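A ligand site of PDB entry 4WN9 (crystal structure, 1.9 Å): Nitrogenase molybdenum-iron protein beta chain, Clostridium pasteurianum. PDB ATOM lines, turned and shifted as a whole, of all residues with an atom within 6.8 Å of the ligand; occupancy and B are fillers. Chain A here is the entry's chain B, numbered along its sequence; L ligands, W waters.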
ATOM      1  N   TYR A  30       7.676 -24.406 -22.545  1.00  0.00           N
ATOM      2  CA  TYR A  30       7.520 -23.666 -21.286  1.00  0.00           C
ATOM      3  C   TYR A  30       7.689 -22.126 -21.478  1.00  0.00           C
ATOM      4  O   TYR A  30       6.890 -21.337 -21.007  1.00  0.00           O
ATOM      5  CB  TYR A  30       8.481 -24.230 -20.233  1.00  0.00           C
ATOM      6  CG  TYR A  30       8.381 -23.584 -18.859  1.00  0.00           C
ATOM      7  CD1 TYR A  30       7.282 -23.793 -18.043  1.00  0.00           C
ATOM      8  CD2 TYR A  30       9.373 -22.727 -18.409  1.00  0.00           C
ATOM      9  CE1 TYR A  30       7.178 -23.175 -16.819  1.00  0.00           C
ATOM     10  CE2 TYR A  30       9.291 -22.115 -17.167  1.00  0.00           C
ATOM     11  CZ  TYR A  30       8.180 -22.326 -16.381  1.00  0.00           C
ATOM     12  OH  TYR A  30       8.121 -21.730 -15.150  1.00  0.00           O
ATOM     13  N   LEU A  56       4.797 -31.185 -18.364  1.00  0.00           N
ATOM     14  CA  LEU A  56       4.336 -29.928 -17.783  1.00  0.00           C
ATOM     15  C   LEU A  56       3.026 -30.166 -17.003  1.00  0.00           C
ATOM     16  O   LEU A  56       2.842 -29.611 -15.924  1.00  0.00           O
ATOM     17  CB  LEU A  56       4.146 -28.864 -18.875  1.00  0.00           C
ATOM     18  CG  LEU A  56       5.457 -28.426 -19.543  1.00  0.00           C
ATOM     19  CD1 LEU A  56       5.161 -27.472 -20.689  1.00  0.00           C
ATOM     20  CD2 LEU A  56       6.415 -27.789 -18.542  1.00  0.00           C
ATOM     21  N   HIS A  59       3.862 -32.028 -13.665  1.00  0.00           N
ATOM     22  CA  HIS A  59       4.555 -31.186 -12.694  1.00  0.00           C
ATOM     23  C   HIS A  59       3.572 -30.212 -12.019  1.00  0.00           C
ATOM     24  O   HIS A  59       3.510 -30.145 -10.781  1.00  0.00           O
ATOM     25  CB  HIS A  59       5.715 -30.439 -13.390  1.00  0.00           C
ATOM     26  CG  HIS A  59       6.399 -29.424 -12.527  1.00  0.00           C
ATOM     27  ND1 HIS A  59       7.631 -29.644 -11.941  1.00  0.00           N
ATOM     28  CD2 HIS A  59       6.020 -28.179 -12.132  1.00  0.00           C
ATOM     29  CE1 HIS A  59       7.972 -28.588 -11.216  1.00  0.00           C
ATOM     30  NE2 HIS A  59       7.019 -27.674 -11.335  1.00  0.00           N
ATOM     31  N   PHE A  60       2.792 -29.486 -12.823  1.00  0.00           N
ATOM     32  CA  PHE A  60       1.985 -28.415 -12.300  1.00  0.00           C
ATOM     33  C   PHE A  60       0.556 -28.810 -11.894  1.00  0.00           C
ATOM     34  O   PHE A  60      -0.117 -28.063 -11.192  1.00  0.00           O
ATOM     35  CB  PHE A  60       1.902 -27.312 -13.349  1.00  0.00           C
ATOM     36  CG  PHE A  60       3.170 -26.565 -13.501  1.00  0.00           C
ATOM     37  CD1 PHE A  60       3.559 -25.636 -12.559  1.00  0.00           C
ATOM     38  CD2 PHE A  60       3.987 -26.800 -14.581  1.00  0.00           C
ATOM     39  CE1 PHE A  60       4.727 -24.950 -12.694  1.00  0.00           C
ATOM     40  CE2 PHE A  60       5.161 -26.091 -14.726  1.00  0.00           C
ATOM     41  CZ  PHE A  60       5.533 -25.176 -13.773  1.00  0.00           C
ATOM     42  N   HIS A 146      16.824 -29.297 -22.279  1.00  0.00           N
ATOM     43  CA  HIS A 146      15.655 -28.458 -22.174  1.00  0.00           C
ATOM     44  C   HIS A 146      15.986 -27.012 -21.726  1.00  0.00           C
ATOM     45  O   HIS A 146      15.295 -26.074 -22.123  1.00  0.00           O
ATOM     46  CB  HIS A 146      14.636 -29.103 -21.226  1.00  0.00           C
ATOM     47  CG  HIS A 146      15.128 -29.211 -19.817  1.00  0.00           C
ATOM     48  ND1 HIS A 146      16.061 -30.144 -19.446  1.00  0.00           N
ATOM     49  CD2 HIS A 146      14.843 -28.492 -18.711  1.00  0.00           C
ATOM     50  CE1 HIS A 146      16.333 -29.996 -18.161  1.00  0.00           C
ATOM     51  NE2 HIS A 146      15.618 -28.999 -17.694  1.00  0.00           N
ATOM     52  N   GLY A 177      15.078 -16.897 -16.384  1.00  0.00           N
ATOM     53  CA  GLY A 177      15.674 -18.197 -16.584  1.00  0.00           C
ATOM     54  C   GLY A 177      14.649 -19.306 -16.411  1.00  0.00           C
ATOM     55  O   GLY A 177      13.436 -19.054 -16.317  1.00  0.00           O
ATOM     56  N   PHE A 178      15.154 -20.535 -16.404  1.00  0.00           N
ATOM     57  CA  PHE A 178      14.324 -21.738 -16.315  1.00  0.00           C
ATOM     58  C   PHE A 178      13.939 -21.990 -14.857  1.00  0.00           C
ATOM     59  O   PHE A 178      14.470 -22.901 -14.178  1.00  0.00           O
ATOM     60  CB  PHE A 178      15.025 -22.938 -16.962  1.00  0.00           C
ATOM     61  CG  PHE A 178      14.108 -24.111 -17.178  1.00  0.00           C
ATOM     62  CD1 PHE A 178      13.107 -24.055 -18.112  1.00  0.00           C
ATOM     63  CD2 PHE A 178      14.209 -25.237 -16.370  1.00  0.00           C
ATOM     64  CE1 PHE A 178      12.234 -25.128 -18.300  1.00  0.00           C
ATOM     65  CE2 PHE A 178      13.337 -26.301 -16.528  1.00  0.00           C
ATOM     66  CZ  PHE A 178      12.355 -26.251 -17.503  1.00  0.00           C
ATOM     67  N   VAL A 179      13.030 -21.151 -14.368  1.00  0.00           N
ATOM     68  CA  VAL A 179      12.496 -21.245 -13.009  1.00  0.00           C
ATOM     69  C   VAL A 179      10.964 -21.346 -13.026  1.00  0.00           C
ATOM     70  O   VAL A 179      10.317 -21.080 -14.032  1.00  0.00           O
ATOM     71  CB  VAL A 179      12.917 -20.024 -12.158  1.00  0.00           C
ATOM     72  CG1 VAL A 179      14.427 -19.930 -12.020  1.00  0.00           C
ATOM     73  CG2 VAL A 179      12.334 -18.757 -12.761  1.00  0.00           C
ATOM     74  N   GLY A 180      10.388 -21.729 -11.897  1.00  0.00           N
ATOM     75  CA  GLY A 180       8.959 -21.974 -11.841  1.00  0.00           C
ATOM     76  C   GLY A 180       8.158 -20.669 -11.788  1.00  0.00           C
ATOM     77  O   GLY A 180       8.704 -19.607 -11.487  1.00  0.00           O
ATOM     78  N   PRO A 181       6.872 -20.750 -12.041  1.00  0.00           N
ATOM     79  CA  PRO A 181       6.029 -19.557 -11.865  1.00  0.00           C
ATOM     80  C   PRO A 181       6.050 -18.898 -10.469  1.00  0.00           C
ATOM     81  O   PRO A 181       5.888 -17.659 -10.360  1.00  0.00           O
ATOM     82  CB  PRO A 181       4.612 -20.057 -12.193  1.00  0.00           C
ATOM     83  CG  PRO A 181       4.685 -21.571 -12.118  1.00  0.00           C
ATOM     84  CD  PRO A 181       6.098 -21.911 -12.527  1.00  0.00           C
ATOM     85  N   ALA A 182       6.200 -19.704  -9.412  1.00  0.00           N
ATOM     86  CA  ALA A 182       6.351 -19.153  -8.066  1.00  0.00           C
ATOM     87  C   ALA A 182       7.585 -18.235  -7.933  1.00  0.00           C
ATOM     88  O   ALA A 182       7.576 -17.214  -7.194  1.00  0.00           O
ATOM     89  CB  ALA A 182       6.436 -20.276  -7.037  1.00  0.00           C
ATOM     90  N   ASP A 183       8.632 -18.628  -8.619  1.00  0.00           N
ATOM     91  CA  ASP A 183       9.895 -17.916  -8.630  1.00  0.00           C
ATOM     92  C   ASP A 183       9.733 -16.619  -9.402  1.00  0.00           C
ATOM     93  O   ASP A 183      10.243 -15.596  -8.989  1.00  0.00           O
ATOM     94  CB  ASP A 183      11.001 -18.777  -9.273  1.00  0.00           C
ATOM     95  CG  ASP A 183      11.292 -20.050  -8.479  1.00  0.00           C
ATOM     96  OD1 ASP A 183      11.266 -20.008  -7.224  1.00  0.00           O
ATOM     97  OD2 ASP A 183      11.536 -21.091  -9.114  1.00  0.00           O
ATOM     98  N   THR A 204       5.630 -17.258 -16.744  1.00  0.00           N
ATOM     99  CA  THR A 204       4.550 -18.283 -16.698  1.00  0.00           C
ATOM    100  C   THR A 204       3.583 -18.149 -15.538  1.00  0.00           C
ATOM    101  O   THR A 204       2.613 -18.921 -15.427  1.00  0.00           O
ATOM    102  CB  THR A 204       5.096 -19.728 -16.674  1.00  0.00           C
ATOM    103  OG1 THR A 204       6.018 -19.904 -15.576  1.00  0.00           O
ATOM    104  CG2 THR A 204       5.763 -20.058 -17.995  1.00  0.00           C
ATOM    105  N   LEU A 208       0.714 -21.385 -15.635  1.00  0.00           N
ATOM    106  CA  LEU A 208       0.901 -22.772 -15.185  1.00  0.00           C
ATOM    107  C   LEU A 208       0.648 -22.950 -13.676  1.00  0.00           C
ATOM    108  O   LEU A 208       0.994 -23.986 -13.075  1.00  0.00           O
ATOM    109  CB  LEU A 208       2.297 -23.280 -15.555  1.00  0.00           C
ATOM    110  CG  LEU A 208       2.431 -23.705 -17.020  1.00  0.00           C
ATOM    111  CD1 LEU A 208       3.880 -23.977 -17.451  1.00  0.00           C
ATOM    112  CD2 LEU A 208       1.555 -24.931 -17.229  1.00  0.00           C
ATOM    113  N   ASP A 320      19.361 -28.764 -12.896  1.00  0.00           N
ATOM    114  CA  ASP A 320      19.663 -27.803 -13.933  1.00  0.00           C
ATOM    115  C   ASP A 320      20.742 -26.808 -13.469  1.00  0.00           C
ATOM    116  O   ASP A 320      20.789 -26.415 -12.286  1.00  0.00           O
ATOM    117  CB  ASP A 320      18.372 -27.117 -14.402  1.00  0.00           C
ATOM    118  CG  ASP A 320      17.382 -28.093 -15.002  1.00  0.00           C
ATOM    119  OD1 ASP A 320      17.809 -29.175 -15.449  1.00  0.00           O
ATOM    120  OD2 ASP A 320      16.144 -27.803 -15.026  1.00  0.00           O
ATOM    121  N   GLU A 323      20.284 -23.259 -11.479  1.00  0.00           N
ATOM    122  CA  GLU A 323      19.689 -23.476 -10.167  1.00  0.00           C
ATOM    123  C   GLU A 323      20.646 -24.222  -9.215  1.00  0.00           C
ATOM    124  O   GLU A 323      20.763 -23.878  -8.038  1.00  0.00           O
ATOM    125  CB  GLU A 323      18.361 -24.238 -10.342  1.00  0.00           C
ATOM    126  CG  GLU A 323      17.217 -23.391 -10.910  1.00  0.00           C
ATOM    127  CD  GLU A 323      17.383 -22.946 -12.372  1.00  0.00           C
ATOM    128  OE1 GLU A 323      17.878 -23.722 -13.233  1.00  0.00           O
ATOM    129  OE2 GLU A 323      17.025 -21.786 -12.660  1.00  0.00           O
ATOM    130  N   PHE A 409      13.163 -30.559  -5.729  1.00  0.00           N
ATOM    131  CA  PHE A 409      13.705 -29.260  -6.179  1.00  0.00           C
ATOM    132  C   PHE A 409      13.789 -29.266  -7.688  1.00  0.00           C
ATOM    133  O   PHE A 409      14.094 -30.297  -8.287  1.00  0.00           O
ATOM    134  CB  PHE A 409      15.098 -29.065  -5.541  1.00  0.00           C
ATOM    135  CG  PHE A 409      15.812 -27.786  -5.932  1.00  0.00           C
ATOM    136  CD1 PHE A 409      16.625 -27.736  -7.049  1.00  0.00           C
ATOM    137  CD2 PHE A 409      15.662 -26.648  -5.162  1.00  0.00           C
ATOM    138  CE1 PHE A 409      17.289 -26.558  -7.408  1.00  0.00           C
ATOM    139  CE2 PHE A 409      16.336 -25.469  -5.501  1.00  0.00           C
ATOM    140  CZ  PHE A 409      17.151 -25.429  -6.619  1.00  0.00           C
ATOM    141  N   GLY A 410      13.456 -28.146  -8.319  1.00  0.00           N
ATOM    142  CA  GLY A 410      13.682 -28.006  -9.737  1.00  0.00           C
ATOM    143  C   GLY A 410      12.625 -28.704 -10.562  1.00  0.00           C
ATOM    144  O   GLY A 410      11.448 -28.716 -10.201  1.00  0.00           O
ATOM    145  N   PHE A 411      13.055 -29.326 -11.658  1.00  0.00           N
ATOM    146  CA  PHE A 411      12.151 -29.819 -12.682  1.00  0.00           C
ATOM    147  C   PHE A 411      12.533 -31.183 -13.208  1.00  0.00           C
ATOM    148  O   PHE A 411      13.682 -31.391 -13.538  1.00  0.00           O
ATOM    149  CB  PHE A 411      12.117 -28.796 -13.836  1.00  0.00           C
ATOM    150  CG  PHE A 411      11.370 -29.268 -15.041  1.00  0.00           C
ATOM    151  CD1 PHE A 411      10.002 -29.174 -15.117  1.00  0.00           C
ATOM    152  CD2 PHE A 411      12.054 -29.822 -16.113  1.00  0.00           C
ATOM    153  CE1 PHE A 411       9.335 -29.611 -16.247  1.00  0.00           C
ATOM    154  CE2 PHE A 411      11.395 -30.248 -17.244  1.00  0.00           C
ATOM    155  CZ  PHE A 411      10.026 -30.144 -17.310  1.00  0.00           C
ATOM    156  N   PRO A 412      11.605 -32.137 -13.291  1.00  0.00           N
ATOM    157  CA  PRO A 412      10.205 -31.967 -12.864  1.00  0.00           C
ATOM    158  C   PRO A 412       9.904 -32.598 -11.505  1.00  0.00           C
ATOM    159  O   PRO A 412      10.515 -33.601 -11.112  1.00  0.00           O
ATOM    160  CB  PRO A 412       9.402 -32.695 -13.947  1.00  0.00           C
ATOM    161  CG  PRO A 412      10.325 -33.734 -14.468  1.00  0.00           C
ATOM    162  CD  PRO A 412      11.741 -33.180 -14.320  1.00  0.00           C
ATOM    163  N   ILE A 413       8.954 -32.005 -10.794  1.00  0.00           N
ATOM    164  CA  ILE A 413       8.426 -32.554  -9.559  1.00  0.00           C
ATOM    165  C   ILE A 413       6.986 -32.936  -9.894  1.00  0.00           C
ATOM    166  O   ILE A 413       6.146 -32.070 -10.122  1.00  0.00           O
ATOM    167  CB  ILE A 413       8.440 -31.515  -8.421  1.00  0.00           C
ATOM    168  CG1 ILE A 413       9.882 -31.050  -8.125  1.00  0.00           C
ATOM    169  CG2 ILE A 413       7.818 -32.102  -7.169  1.00  0.00           C
ATOM    170  CD1 ILE A 413       9.998 -29.898  -7.143  1.00  0.00           C
ATOM    171  N   HIS A 419       3.437 -27.646  -4.465  1.00  0.00           N
ATOM    172  CA  HIS A 419       4.809 -27.169  -4.405  1.00  0.00           C
ATOM    173  C   HIS A 419       5.019 -26.013  -5.364  1.00  0.00           C
ATOM    174  O   HIS A 419       5.832 -25.145  -5.103  1.00  0.00           O
ATOM    175  CB  HIS A 419       5.792 -28.293  -4.740  1.00  0.00           C
ATOM    176  CG  HIS A 419       5.589 -28.894  -6.094  1.00  0.00           C
ATOM    177  ND1 HIS A 419       6.174 -28.398  -7.233  1.00  0.00           N
ATOM    178  CD2 HIS A 419       4.867 -29.967  -6.473  1.00  0.00           C
ATOM    179  CE1 HIS A 419       5.803 -29.128  -8.265  1.00  0.00           C
ATOM    180  NE2 HIS A 419       5.014 -30.096  -7.827  1.00  0.00           N
ATOM    181  N   TYR A 420       4.247 -25.983  -6.454  1.00  0.00           N
ATOM    182  CA  TYR A 420       4.392 -24.939  -7.459  1.00  0.00           C
ATOM    183  C   TYR A 420       3.849 -23.595  -6.962  1.00  0.00           C
ATOM    184  O   TYR A 420       3.902 -22.615  -7.701  1.00  0.00           O
ATOM    185  CB  TYR A 420       3.718 -25.354  -8.789  1.00  0.00           C
ATOM    186  CG  TYR A 420       2.547 -26.248  -8.515  1.00  0.00           C
ATOM    187  CD1 TYR A 420       1.336 -25.728  -8.098  1.00  0.00           C
ATOM    188  CD2 TYR A 420       2.677 -27.616  -8.573  1.00  0.00           C
ATOM    189  CE1 TYR A 420       0.277 -26.541  -7.770  1.00  0.00           C
ATOM    190  CE2 TYR A 420       1.609 -28.441  -8.245  1.00  0.00           C
ATOM    191  CZ  TYR A 420       0.419 -27.876  -7.839  1.00  0.00           C
ATOM    192  OH  TYR A 420      -0.629 -28.687  -7.492  1.00  0.00           O
ATOM    193  N   ASN A 422       5.232 -22.272  -4.231  1.00  0.00           N
ATOM    194  CA  ASN A 422       6.296 -21.859  -3.329  1.00  0.00           C
ATOM    195  C   ASN A 422       7.573 -21.527  -4.045  1.00  0.00           C
ATOM    196  O   ASN A 422       8.084 -22.353  -4.797  1.00  0.00           O
ATOM    197  CB  ASN A 422       6.612 -22.969  -2.315  1.00  0.00           C
ATOM    198  CG  ASN A 422       5.461 -23.231  -1.356  1.00  0.00           C
ATOM    199  OD1 ASN A 422       4.715 -22.319  -0.979  1.00  0.00           O
ATOM    200  ND2 ASN A 422       5.307 -24.499  -0.953  1.00  0.00           N
ATOM    201  N   LYS A 424      11.614 -20.920  -4.578  1.00  0.00           N
ATOM    202  CA  LYS A 424      12.932 -21.235  -4.038  1.00  0.00           C
ATOM    203  C   LYS A 424      13.873 -20.022  -4.114  1.00  0.00           C
ATOM    204  O   LYS A 424      14.904 -20.026  -3.493  1.00  0.00           O
ATOM    205  CB  LYS A 424      13.565 -22.395  -4.821  1.00  0.00           C
ATOM    206  CG  LYS A 424      13.612 -22.205  -6.326  1.00  0.00           C
ATOM    207  CD  LYS A 424      14.232 -23.419  -7.008  1.00  0.00           C
ATOM    208  CE  LYS A 424      13.945 -23.454  -8.492  1.00  0.00           C
ATOM    209  NZ  LYS A 424      12.504 -23.584  -8.756  1.00  0.00           N
HETATM  210  N1  LIG L   1       9.259 -25.544 -13.198  1.00  0.00           N
HETATM  211  C1  LIG L   1      10.651 -25.487 -12.811  1.00  0.00           C
HETATM  212  C2  LIG L   1      10.935 -24.932 -11.434  1.00  0.00           C
HETATM  213  O1  LIG L   1      10.089 -24.933 -10.524  1.00  0.00           O
HETATM  214  C3  LIG L   1      11.255 -24.642 -13.920  1.00  0.00           C
HETATM  215  C4  LIG L   1      10.378 -24.913 -15.125  1.00  0.00           C
HETATM  216  C5  LIG L   1       9.154 -25.617 -14.665  1.00  0.00           C
HETATM  217  O2  LIG L   1      12.054 -24.515 -11.217  1.00  0.00           O
HETATM  218  O   HOH W   1       7.262 -25.150 -10.102  1.00  0.00           O
HETATM  219  O   HOH W   2      10.251 -26.719  -8.663  1.00  0.00           O
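The side-chain amino group (NZ) of Lys 424 is in salt-bridge range of an oxygen (O2) of the ligand, at 2.7 Å. O2 of the ligand sits close to N of Gly 180.
The side-chain amino group (NZ) of Lys 424 lies within salt-bridge range of the side-chain carboxylate (OD2) of Asp 183, at 2.7 Å. N of Gly 180 sits at hydrogen-bond distance from OD2 of Asp 183 (3.1 Å). O of Val 179 sits at hydrogen-bond distance from OH of Tyr 30 (2.5 Å). A ring nitrogen (ND1) of His 59 sits at hydrogen-bond distance from the backbone NH (N) of Ile 413 (2.9 Å). O of His 59 is in hydrogen-bond range of NE2 of His 419. OG1 of Thr 204 lies within hydrogen-bond range of OH of Tyr 30 (2.8 Å).
Residues that only touch the ligand: Phe 178 (3.4 Å), Val 179 (3.4 Å), His 59 (3.6 Å), Tyr 30 (3.6 Å), Phe 411 (3.7 Å) and Phe 60 (3.8 Å). Hydrophobic or aromatic side chains within 4 Å of the ligand: Tyr 30, His 59, Phe 60, Phe 178 and Phe 411. The nearest printed residue that does not touch the ligand is Gly 410 (4.01 Å).
Water W2 lies within hydrogen-bond range of an oxygen (O1) of the ligand (2.6 Å) and the backbone carbonyl oxygen (O) of Gly 410 (2.8 Å). Water W1 bridges a ring nitrogen (NE2) of His 59 (2.8 Å) and an oxygen (O1) of the ligand (2.9 Å).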
